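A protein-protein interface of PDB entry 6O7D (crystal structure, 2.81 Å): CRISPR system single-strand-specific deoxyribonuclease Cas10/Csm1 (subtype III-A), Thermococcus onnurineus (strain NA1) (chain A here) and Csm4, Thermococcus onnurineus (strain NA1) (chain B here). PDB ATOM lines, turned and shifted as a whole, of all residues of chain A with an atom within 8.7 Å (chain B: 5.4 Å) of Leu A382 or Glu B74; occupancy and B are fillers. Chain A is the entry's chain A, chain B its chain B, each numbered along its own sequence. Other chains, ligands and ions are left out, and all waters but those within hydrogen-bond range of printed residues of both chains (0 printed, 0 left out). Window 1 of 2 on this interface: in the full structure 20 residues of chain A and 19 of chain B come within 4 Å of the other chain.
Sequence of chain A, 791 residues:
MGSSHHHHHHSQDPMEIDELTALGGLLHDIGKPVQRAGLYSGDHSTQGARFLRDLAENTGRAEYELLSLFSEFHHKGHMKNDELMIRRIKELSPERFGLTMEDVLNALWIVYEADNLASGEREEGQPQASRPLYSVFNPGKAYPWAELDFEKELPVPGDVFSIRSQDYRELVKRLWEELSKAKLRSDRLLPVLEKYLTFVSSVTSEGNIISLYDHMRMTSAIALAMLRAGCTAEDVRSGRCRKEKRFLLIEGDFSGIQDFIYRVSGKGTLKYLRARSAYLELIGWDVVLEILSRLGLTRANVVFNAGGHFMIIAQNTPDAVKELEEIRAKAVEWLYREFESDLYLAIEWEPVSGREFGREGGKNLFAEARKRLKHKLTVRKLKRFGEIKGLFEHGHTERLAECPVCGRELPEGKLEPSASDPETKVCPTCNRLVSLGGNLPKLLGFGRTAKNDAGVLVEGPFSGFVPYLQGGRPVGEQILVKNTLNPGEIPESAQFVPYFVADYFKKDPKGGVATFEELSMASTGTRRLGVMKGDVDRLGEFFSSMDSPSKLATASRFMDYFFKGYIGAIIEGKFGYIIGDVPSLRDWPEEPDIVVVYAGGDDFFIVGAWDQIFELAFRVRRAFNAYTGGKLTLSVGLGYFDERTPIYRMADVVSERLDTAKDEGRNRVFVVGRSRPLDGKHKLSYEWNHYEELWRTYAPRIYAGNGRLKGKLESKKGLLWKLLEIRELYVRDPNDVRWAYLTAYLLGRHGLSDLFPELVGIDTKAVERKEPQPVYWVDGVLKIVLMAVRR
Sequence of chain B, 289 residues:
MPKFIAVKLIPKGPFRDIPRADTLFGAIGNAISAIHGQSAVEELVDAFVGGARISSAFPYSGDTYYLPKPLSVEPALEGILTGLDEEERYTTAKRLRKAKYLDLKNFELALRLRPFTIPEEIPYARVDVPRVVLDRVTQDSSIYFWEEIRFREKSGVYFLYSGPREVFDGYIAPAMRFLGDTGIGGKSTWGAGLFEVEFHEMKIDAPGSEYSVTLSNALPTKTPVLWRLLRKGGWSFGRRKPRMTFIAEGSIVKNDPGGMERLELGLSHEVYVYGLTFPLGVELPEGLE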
ATOM      1  N   SER A 255       7.074   6.651  14.399  1.00  0.00           N
ATOM      2  CA  SER A 255       5.822   7.451  14.325  1.00  0.00           C
ATOM      3  C   SER A 255       6.151   8.941  14.484  1.00  0.00           C
ATOM      4  O   SER A 255       6.846   9.291  15.460  1.00  0.00           O
ATOM      5  CB  SER A 255       4.819   6.990  15.353  1.00  0.00           C
ATOM      6  OG  SER A 255       5.030   7.633  16.601  1.00  0.00           O
ATOM      7  N   TYR A 344       8.853   9.061  18.008  1.00  0.00           N
ATOM      8  CA  TYR A 344       8.706   7.796  18.772  1.00  0.00           C
ATOM      9  C   TYR A 344       9.118   6.619  17.883  1.00  0.00           C
ATOM     10  O   TYR A 344       8.904   6.698  16.654  1.00  0.00           O
ATOM     11  CB  TYR A 344       7.262   7.631  19.253  1.00  0.00           C
ATOM     12  CG  TYR A 344       6.998   6.342  19.987  1.00  0.00           C
ATOM     13  CD1 TYR A 344       7.696   6.030  21.143  1.00  0.00           C
ATOM     14  CD2 TYR A 344       6.063   5.430  19.529  1.00  0.00           C
ATOM     15  CE1 TYR A 344       7.470   4.847  21.826  1.00  0.00           C
ATOM     16  CE2 TYR A 344       5.821   4.243  20.203  1.00  0.00           C
ATOM     17  CZ  TYR A 344       6.526   3.952  21.356  1.00  0.00           C
ATOM     18  OH  TYR A 344       6.296   2.788  22.027  1.00  0.00           O
ATOM     19  N   ALA A 346       8.175   2.705  17.686  1.00  0.00           N
ATOM     20  CA  ALA A 346       7.318   1.551  18.043  1.00  0.00           C
ATOM     21  C   ALA A 346       7.995   0.261  17.565  1.00  0.00           C
ATOM     22  O   ALA A 346       7.933  -0.022  16.352  1.00  0.00           O
ATOM     23  CB  ALA A 346       5.945   1.718  17.437  1.00  0.00           C
ATOM     24  N   HIS A 375      -0.794  -5.267  13.980  1.00  0.00           N
ATOM     25  CA  HIS A 375      -1.751  -4.954  15.074  1.00  0.00           C
ATOM     26  C   HIS A 375      -0.980  -4.609  16.354  1.00  0.00           C
ATOM     27  O   HIS A 375      -1.337  -3.604  16.998  1.00  0.00           O
ATOM     28  CB  HIS A 375      -2.737  -6.108  15.298  1.00  0.00           C
ATOM     29  CG  HIS A 375      -3.817  -5.775  16.272  1.00  0.00           C
ATOM     30  ND1 HIS A 375      -3.830  -6.276  17.560  1.00  0.00           N
ATOM     31  CD2 HIS A 375      -4.900  -4.977  16.162  1.00  0.00           C
ATOM     32  CE1 HIS A 375      -4.886  -5.810  18.198  1.00  0.00           C
ATOM     33  NE2 HIS A 375      -5.558  -5.010  17.362  1.00  0.00           N
ATOM     34  N   LYS A 376       0.029  -5.412  16.711  1.00  0.00           N
ATOM     35  CA  LYS A 376       0.896  -5.171  17.898  1.00  0.00           C
ATOM     36  C   LYS A 376       1.510  -3.767  17.794  1.00  0.00           C
ATOM     37  O   LYS A 376       1.619  -3.099  18.843  1.00  0.00           O
ATOM     38  CB  LYS A 376       1.986  -6.242  18.032  1.00  0.00           C
ATOM     39  CG  LYS A 376       1.541  -7.580  18.613  1.00  0.00           C
ATOM     40  CD  LYS A 376       2.502  -8.146  19.653  1.00  0.00           C
ATOM     41  CE  LYS A 376       2.904  -9.587  19.404  1.00  0.00           C
ATOM     42  NZ  LYS A 376       1.805 -10.536  19.700  1.00  0.00           N
ATOM     43  N   LEU A 377       1.883  -3.338  16.580  1.00  0.00           N
ATOM     44  CA  LEU A 377       2.488  -2.003  16.301  1.00  0.00           C
ATOM     45  C   LEU A 377       1.436  -0.901  16.484  1.00  0.00           C
ATOM     46  O   LEU A 377       1.716   0.047  17.246  1.00  0.00           O
ATOM     47  CB  LEU A 377       3.065  -1.967  14.881  1.00  0.00           C
ATOM     48  CG  LEU A 377       4.451  -2.584  14.695  1.00  0.00           C
ATOM     49  CD1 LEU A 377       4.848  -2.562  13.227  1.00  0.00           C
ATOM     50  CD2 LEU A 377       5.497  -1.864  15.531  1.00  0.00           C
ATOM     51  N   THR A 378       0.288  -1.009  15.803  1.00  0.00           N
ATOM     52  CA  THR A 378      -0.833  -0.029  15.870  1.00  0.00           C
ATOM     53  C   THR A 378      -1.152   0.281  17.338  1.00  0.00           C
ATOM     54  O   THR A 378      -1.334   1.470  17.657  1.00  0.00           O
ATOM     55  CB  THR A 378      -2.100  -0.525  15.158  1.00  0.00           C
ATOM     56  OG1 THR A 378      -2.390  -1.843  15.623  1.00  0.00           O
ATOM     57  CG2 THR A 378      -1.981  -0.531  13.650  1.00  0.00           C
ATOM     58  N   VAL A 379      -1.210  -0.751  18.186  1.00  0.00           N
ATOM     59  CA  VAL A 379      -1.497  -0.635  19.648  1.00  0.00           C
ATOM     60  C   VAL A 379      -0.330   0.091  20.330  1.00  0.00           C
ATOM     61  O   VAL A 379      -0.602   0.998  21.140  1.00  0.00           O
ATOM     62  CB  VAL A 379      -1.761  -2.013  20.290  1.00  0.00           C
ATOM     63  CG1 VAL A 379      -1.800  -1.941  21.810  1.00  0.00           C
ATOM     64  CG2 VAL A 379      -3.040  -2.641  19.759  1.00  0.00           C
ATOM     65  N   ARG A 380       0.914  -0.288  20.016  1.00  0.00           N
ATOM     66  CA  ARG A 380       2.138   0.313  20.615  1.00  0.00           C
ATOM     67  C   ARG A 380       2.240   1.788  20.196  1.00  0.00           C
ATOM     68  O   ARG A 380       2.796   2.582  20.982  1.00  0.00           O
ATOM     69  CB  ARG A 380       3.387  -0.488  20.223  1.00  0.00           C
ATOM     70  CG  ARG A 380       4.684   0.008  20.849  1.00  0.00           C
ATOM     71  CD  ARG A 380       4.653   0.083  22.366  1.00  0.00           C
ATOM     72  NE  ARG A 380       4.756  -1.220  23.011  1.00  0.00           N
ATOM     73  CZ  ARG A 380       4.564  -1.448  24.311  1.00  0.00           C
ATOM     74  NH1 ARG A 380       4.239  -0.457  25.129  1.00  0.00           N
ATOM     75  NH2 ARG A 380       4.691  -2.674  24.789  1.00  0.00           N
ATOM     76  N   LYS A 381       1.709   2.138  19.018  1.00  0.00           N
ATOM     77  CA  LYS A 381       1.661   3.532  18.490  1.00  0.00           C
ATOM     78  C   LYS A 381       0.561   4.341  19.193  1.00  0.00           C
ATOM     79  O   LYS A 381       0.595   5.580  19.082  1.00  0.00           O
ATOM     80  CB  LYS A 381       1.407   3.542  16.980  1.00  0.00           C
ATOM     81  CG  LYS A 381       2.620   3.246  16.110  1.00  0.00           C
ATOM     82  CD  LYS A 381       2.369   3.537  14.647  1.00  0.00           C
ATOM     83  CE  LYS A 381       3.110   2.600  13.718  1.00  0.00           C
ATOM     84  NZ  LYS A 381       3.041   3.065  12.314  1.00  0.00           N
ATOM     85  N   LEU A 382      -0.395   3.671  19.848  1.00  0.00           N
ATOM     86  CA  LEU A 382      -1.463   4.309  20.667  1.00  0.00           C
ATOM     87  C   LEU A 382      -1.074   4.262  22.151  1.00  0.00           C
ATOM     88  O   LEU A 382      -1.923   4.610  22.994  1.00  0.00           O
ATOM     89  CB  LEU A 382      -2.792   3.589  20.414  1.00  0.00           C
ATOM     90  CG  LEU A 382      -3.368   3.741  19.007  1.00  0.00           C
ATOM     91  CD1 LEU A 382      -4.629   2.910  18.848  1.00  0.00           C
ATOM     92  CD2 LEU A 382      -3.650   5.200  18.679  1.00  0.00           C
ATOM     93  N   LYS A 383       0.163   3.848  22.446  1.00  0.00           N
ATOM     94  CA  LYS A 383       0.768   3.847  23.805  1.00  0.00           C
ATOM     95  C   LYS A 383       2.161   4.483  23.708  1.00  0.00           C
ATOM     96  O   LYS A 383       3.122   3.898  24.246  1.00  0.00           O
ATOM     97  CB  LYS A 383       0.816   2.416  24.354  1.00  0.00           C
ATOM     98  CG  LYS A 383      -0.528   1.699  24.421  1.00  0.00           C
ATOM     99  CD  LYS A 383      -0.422   0.211  24.689  1.00  0.00           C
ATOM    100  CE  LYS A 383       0.042  -0.122  26.092  1.00  0.00           C
ATOM    101  NZ  LYS A 383      -1.032   0.083  27.093  1.00  0.00           N
ATOM    102  N   ARG A 384       2.248   5.641  23.041  1.00  0.00           N
ATOM    103  CA  ARG A 384       3.520   6.334  22.695  1.00  0.00           C
ATOM    104  C   ARG A 384       4.242   6.767  23.975  1.00  0.00           C
ATOM    105  O   ARG A 384       3.676   7.582  24.728  1.00  0.00           O
ATOM    106  CB  ARG A 384       3.259   7.532  21.774  1.00  0.00           C
ATOM    107  CG  ARG A 384       3.003   7.144  20.324  1.00  0.00           C
ATOM    108  CD  ARG A 384       2.926   8.315  19.360  1.00  0.00           C
ATOM    109  NE  ARG A 384       4.131   9.137  19.353  1.00  0.00           N
ATOM    110  CZ  ARG A 384       4.338  10.181  18.552  1.00  0.00           C
ATOM    111  NH1 ARG A 384       3.418  10.548  17.675  1.00  0.00           N
ATOM    112  NH2 ARG A 384       5.472  10.856  18.634  1.00  0.00           N
ATOM    113  N   PHE A 385       5.446   6.227  24.193  1.00  0.00           N
ATOM    114  CA  PHE A 385       6.354   6.501  25.342  1.00  0.00           C
ATOM    115  C   PHE A 385       5.796   5.853  26.617  1.00  0.00           C
ATOM    116  O   PHE A 385       6.133   6.319  27.723  1.00  0.00           O
ATOM    117  CB  PHE A 385       6.595   8.005  25.496  1.00  0.00           C
ATOM    118  CG  PHE A 385       7.290   8.636  24.317  1.00  0.00           C
ATOM    119  CD1 PHE A 385       8.669   8.563  24.186  1.00  0.00           C
ATOM    120  CD2 PHE A 385       6.569   9.292  23.332  1.00  0.00           C
ATOM    121  CE1 PHE A 385       9.310   9.140  23.102  1.00  0.00           C
ATOM    122  CE2 PHE A 385       7.212   9.865  22.245  1.00  0.00           C
ATOM    123  CZ  PHE A 385       8.581   9.789  22.133  1.00  0.00           C
ATOM    124  N   GLY A 386       5.006   4.784  26.462  1.00  0.00           N
ATOM    125  CA  GLY A 386       4.473   3.966  27.569  1.00  0.00           C
ATOM    126  C   GLY A 386       5.562   3.162  28.262  1.00  0.00           C
ATOM    127  O   GLY A 386       5.308   2.680  29.384  1.00  0.00           O
ATOM    128  N   LYS B  69     -13.799  10.992  18.458  1.00  0.00           N
ATOM    129  CA  LYS B  69     -13.587   9.561  18.118  1.00  0.00           C
ATOM    130  C   LYS B  69     -12.773   8.905  19.230  1.00  0.00           C
ATOM    131  O   LYS B  69     -11.628   9.291  19.458  1.00  0.00           O
ATOM    132  CB  LYS B  69     -12.854   9.468  16.775  1.00  0.00           C
ATOM    133  CG  LYS B  69     -12.444   8.070  16.327  1.00  0.00           C
ATOM    134  CD  LYS B  69     -11.247   8.087  15.401  1.00  0.00           C
ATOM    135  CE  LYS B  69     -10.831   6.712  14.926  1.00  0.00           C
ATOM    136  NZ  LYS B  69     -11.861   6.101  14.053  1.00  0.00           N
ATOM    137  N   PRO B  70     -13.327   7.916  19.971  1.00  0.00           N
ATOM    138  CA  PRO B  70     -12.555   7.216  20.997  1.00  0.00           C
ATOM    139  C   PRO B  70     -11.474   6.335  20.355  1.00  0.00           C
ATOM    140  O   PRO B  70     -11.767   5.668  19.379  1.00  0.00           O
ATOM    141  CB  PRO B  70     -13.600   6.379  21.750  1.00  0.00           C
ATOM    142  CG  PRO B  70     -14.718   6.179  20.746  1.00  0.00           C
ATOM    143  CD  PRO B  70     -14.707   7.415  19.869  1.00  0.00           C
ATOM    144  N   LEU B  71     -10.262   6.352  20.922  1.00  0.00           N
ATOM    145  CA  LEU B  71      -9.083   5.593  20.423  1.00  0.00           C
ATOM    146  C   LEU B  71      -9.324   4.083  20.566  1.00  0.00           C
ATOM    147  O   LEU B  71      -8.484   3.310  20.069  1.00  0.00           O
ATOM    148  CB  LEU B  71      -7.836   6.032  21.200  1.00  0.00           C
ATOM    149  CG  LEU B  71      -7.383   7.475  20.978  1.00  0.00           C
ATOM    150  CD1 LEU B  71      -6.110   7.768  21.759  1.00  0.00           C
ATOM    151  CD2 LEU B  71      -7.172   7.766  19.500  1.00  0.00           C
ATOM    152  N   SER B  72     -10.425   3.684  21.216  1.00  0.00           N
ATOM    153  CA  SER B  72     -10.835   2.272  21.444  1.00  0.00           C
ATOM    154  C   SER B  72     -11.081   1.546  20.116  1.00  0.00           C
ATOM    155  O   SER B  72     -10.788   0.337  20.057  1.00  0.00           O
ATOM    156  CB  SER B  72     -12.053   2.204  22.331  1.00  0.00           C
ATOM    157  OG  SER B  72     -13.190   2.749  21.678  1.00  0.00           O
ATOM    158  N   VAL B  73     -11.611   2.240  19.101  1.00  0.00           N
ATOM    159  CA  VAL B  73     -12.036   1.626  17.804  1.00  0.00           C
ATOM    160  C   VAL B  73     -10.811   1.404  16.908  1.00  0.00           C
ATOM    161  O   VAL B  73     -10.897   0.520  16.035  1.00  0.00           O
ATOM    162  CB  VAL B  73     -13.109   2.460  17.074  1.00  0.00           C
ATOM    163  CG1 VAL B  73     -14.300   2.765  17.969  1.00  0.00           C
ATOM    164  CG2 VAL B  73     -12.548   3.739  16.471  1.00  0.00           C
ATOM    165  N   GLU B  74      -9.729   2.166  17.114  1.00  0.00           N
ATOM    166  CA  GLU B  74      -8.519   2.169  16.240  1.00  0.00           C
ATOM    167  C   GLU B  74      -8.015   0.739  16.048  1.00  0.00           C
ATOM    168  O   GLU B  74      -7.817   0.311  14.913  1.00  0.00           O
ATOM    169  CB  GLU B  74      -7.408   3.062  16.806  1.00  0.00           C
ATOM    170  CG  GLU B  74      -7.771   4.532  16.928  1.00  0.00           C
ATOM    171  CD  GLU B  74      -7.789   5.305  15.621  1.00  0.00           C
ATOM    172  OE1 GLU B  74      -8.306   4.765  14.626  1.00  0.00           O
ATOM    173  OE2 GLU B  74      -7.283   6.445  15.604  1.00  0.00           O
ATOM    174  N   PRO B  75      -7.793  -0.050  17.129  1.00  0.00           N
ATOM    175  CA  PRO B  75      -7.314  -1.429  16.997  1.00  0.00           C
ATOM    176  C   PRO B  75      -8.387  -2.474  16.636  1.00  0.00           C
ATOM    177  O   PRO B  75      -8.026  -3.627  16.491  1.00  0.00           O
ATOM    178  CB  PRO B  75      -6.763  -1.762  18.399  1.00  0.00           C
ATOM    179  CG  PRO B  75      -6.812  -0.455  19.174  1.00  0.00           C
ATOM    180  CD  PRO B  75      -7.936   0.331  18.540  1.00  0.00           C
ATOM    181  N   ALA B  76      -9.654  -2.063  16.502  1.00  0.00           N
ATOM    182  CA  ALA B  76     -10.829  -2.954  16.340  1.00  0.00           C
ATOM    183  C   ALA B  76     -11.509  -2.743  14.980  1.00  0.00           C
ATOM    184  O   ALA B  76     -12.611  -3.297  14.793  1.00  0.00           O
ATOM    185  CB  ALA B  76     -11.805  -2.702  17.461  1.00  0.00           C
ATOM    186  N   LEU B  77     -10.884  -1.994  14.064  1.00  0.00           N
ATOM    187  CA  LEU B  77     -11.516  -1.544  12.791  1.00  0.00           C
ATOM    188  C   LEU B  77     -11.804  -2.740  11.871  1.00  0.00           C
ATOM    189  O   LEU B  77     -12.640  -2.579  10.960  1.00  0.00           O
ATOM    190  CB  LEU B  77     -10.611  -0.514  12.107  1.00  0.00           C
ATOM    191  CG  LEU B  77     -10.531   0.845  12.803  1.00  0.00           C
ATOM    192  CD1 LEU B  77      -9.363   1.664  12.277  1.00  0.00           C
ATOM    193  CD2 LEU B  77     -11.832   1.617  12.650  1.00  0.00           C
ATOM    194  N   LEU B  96     -11.210   6.353   8.680  1.00  0.00           N
ATOM    195  CA  LEU B  96     -11.736   6.263  10.072  1.00  0.00           C
ATOM    196  C   LEU B  96     -10.609   6.645  11.040  1.00  0.00           C
ATOM    197  O   LEU B  96     -10.866   7.441  11.961  1.00  0.00           O
ATOM    198  CB  LEU B  96     -12.241   4.846  10.373  1.00  0.00           C
ATOM    199  CG  LEU B  96     -13.222   4.232   9.372  1.00  0.00           C
ATOM    200  CD1 LEU B  96     -13.471   2.765   9.685  1.00  0.00           C
ATOM    201  CD2 LEU B  96     -14.537   4.987   9.343  1.00  0.00           C
ATOM    202  N   ARG B  97      -9.407   6.102  10.811  1.00  0.00           N
ATOM    203  CA  ARG B  97      -8.197   6.285  11.661  1.00  0.00           C
ATOM    204  C   ARG B  97      -7.768   7.760  11.666  1.00  0.00           C
ATOM    205  O   ARG B  97      -7.062   8.157  12.614  1.00  0.00           O
ATOM    206  CB  ARG B  97      -7.064   5.378  11.163  1.00  0.00           C
ATOM    207  CG  ARG B  97      -5.965   5.111  12.183  1.00  0.00           C
ATOM    208  CD  ARG B  97      -4.828   4.287  11.606  1.00  0.00           C
ATOM    209  NE  ARG B  97      -5.220   2.925  11.260  1.00  0.00           N
ATOM    210  CZ  ARG B  97      -5.307   1.905  12.114  1.00  0.00           C
ATOM    211  NH1 ARG B  97      -5.669   0.709  11.675  1.00  0.00           N
ATOM    212  NH2 ARG B  97      -5.039   2.072  13.399  1.00  0.00           N
ATOM    213  N   VAL B 225      -4.563   3.377  29.025  1.00  0.00           N
ATOM    214  CA  VAL B 225      -4.746   2.187  28.138  1.00  0.00           C
ATOM    215  C   VAL B 225      -4.326   2.574  26.713  1.00  0.00           C
ATOM    216  O   VAL B 225      -3.274   2.084  26.262  1.00  0.00           O
ATOM    217  CB  VAL B 225      -6.192   1.654  28.190  1.00  0.00           C
ATOM    218  CG1 VAL B 225      -6.330   0.332  27.451  1.00  0.00           C
ATOM    219  CG2 VAL B 225      -6.697   1.516  29.618  1.00  0.00           C
ATOM    220  N   LEU B 226      -5.121   3.419  26.045  1.00  0.00           N
ATOM    221  CA  LEU B 226      -4.845   3.986  24.696  1.00  0.00           C
ATOM    222  C   LEU B 226      -4.842   5.513  24.816  1.00  0.00           C
ATOM    223  O   LEU B 226      -5.720   6.039  25.527  1.00  0.00           O
ATOM    224  CB  LEU B 226      -5.928   3.523  23.716  1.00  0.00           C
ATOM    225  CG  LEU B 226      -6.112   2.012  23.586  1.00  0.00           C
ATOM    226  CD1 LEU B 226      -7.380   1.690  22.812  1.00  0.00           C
ATOM    227  CD2 LEU B 226      -4.903   1.367  22.924  1.00  0.00           C
ATOM    228  N   TRP B 227      -3.903   6.202  24.162  1.00  0.00           N
ATOM    229  CA  TRP B 227      -3.733   7.669  24.334  1.00  0.00           C
ATOM    230  C   TRP B 227      -2.933   8.296  23.186  1.00  0.00           C
ATOM    231  O   TRP B 227      -2.213   7.564  22.476  1.00  0.00           O
ATOM    232  CB  TRP B 227      -3.087   7.963  25.692  1.00  0.00           C
ATOM    233  CG  TRP B 227      -1.603   7.753  25.762  1.00  0.00           C
ATOM    234  CD1 TRP B 227      -0.634   8.638  25.387  1.00  0.00           C
ATOM    235  CD2 TRP B 227      -0.911   6.602  26.284  1.00  0.00           C
ATOM    236  NE1 TRP B 227       0.607   8.115  25.624  1.00  0.00           N
ATOM    237  CE2 TRP B 227       0.471   6.870  26.177  1.00  0.00           C
ATOM    238  CE3 TRP B 227      -1.316   5.375  26.824  1.00  0.00           C
ATOM    239  CZ2 TRP B 227       1.442   5.957  26.590  1.00  0.00           C
ATOM    240  CZ3 TRP B 227      -0.357   4.476  27.237  1.00  0.00           C
ATOM    241  CH2 TRP B 227       1.003   4.763  27.117  1.00  0.00           C
ATOM    242  N   ARG B 228      -3.081   9.616  23.035  1.00  0.00           N
ATOM    243  CA  ARG B 228      -2.211  10.499  22.216  1.00  0.00           C
ATOM    244  C   ARG B 228      -1.670  11.608  23.123  1.00  0.00           C
ATOM    245  O   ARG B 228      -2.490  12.366  23.680  1.00  0.00           O
ATOM    246  CB  ARG B 228      -2.987  11.089  21.034  1.00  0.00           C
ATOM    247  CG  ARG B 228      -3.501  10.052  20.045  1.00  0.00           C
ATOM    248  CD  ARG B 228      -3.910  10.644  18.708  1.00  0.00           C
ATOM    249  NE  ARG B 228      -4.325  12.042  18.795  1.00  0.00           N
ATOM    250  CZ  ARG B 228      -5.534  12.474  19.159  1.00  0.00           C
ATOM    251  NH1 ARG B 228      -5.780  13.773  19.196  1.00  0.00           N
ATOM    252  NH2 ARG B 228      -6.490  11.621  19.487  1.00  0.00           N
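Of the printed residues of chain B, His A375 touches Pro B75 (3.0 Å).
Of the printed residues of chain B, Arg A384 touches Trp B227.
Of the printed residues of chain B, Gly A386 touches Trp B227 (3.6 Å).
Lys B69 touches none of the printed residues of chain A.
Glu B74 touches just one residue of chain A: Leu A382 (3.5 Å).
Of the printed residues of chain A, Val B225 touches Lys A383.
Of the printed residues of chain A, Leu B226 touches Leu A382.
The nearest residue of chain B that does not touch Leu A382 is Pro B75 (4.02 Å).
The nearest residue of chain A that does not touch Glu B74 is Thr A378 (5.8 Å).
The nearest printed residue of chain A that does not touch Trp B227 is Phe A385 (4.4 Å).
The side-chain hydroxyl (OG) of Ser A255 sits at hydrogen-bond distance from the guanidinium group (NE) of Arg A384 (3.3 Å).
O of His A375 is in hydrogen-bond range of OG1 of Thr A378 (2.5 Å).
The side-chain amino group of Lys B69 lies within salt-bridge range of the side-chain carboxylate of Glu B74, 3.8 Å away.
Among the printed residues, merely in contact across the chains: Lys A383 with Trp B227 (3.3 Å), Leu A382 with Leu B226 (3.4 Å), Leu A382 with Glu B74 (3.5 Å) and Gly A386 with Trp B227 (3.6 Å).
Hydrophobic or aromatic side chains of chain A that line the printed part of chain B: His A375 and Leu A382.
Hydrophobic or aromatic side chains of chain B that line the printed part of chain A: Pro B75, Leu B226 and Trp B227.
Among the printed residues, no Asp or Glu carboxylate lies within 4 Å of a Lys or Arg side-chain nitrogen of the other chain.
NE2 of His A375 lies within hydrogen-bond range of O of Pro B75 (3.0 Å).
O of Leu A382 is in hydrogen-bond range of N of Trp B227 (2.8 Å).
NZ of Lys A383 lies within hydrogen-bond range of O of Val B225, at 3.1 Å.
The backbone carbonyl oxygen of Arg A384 is in hydrogen-bond range of the indole nitrogen of Trp B227 (3.2 Å).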
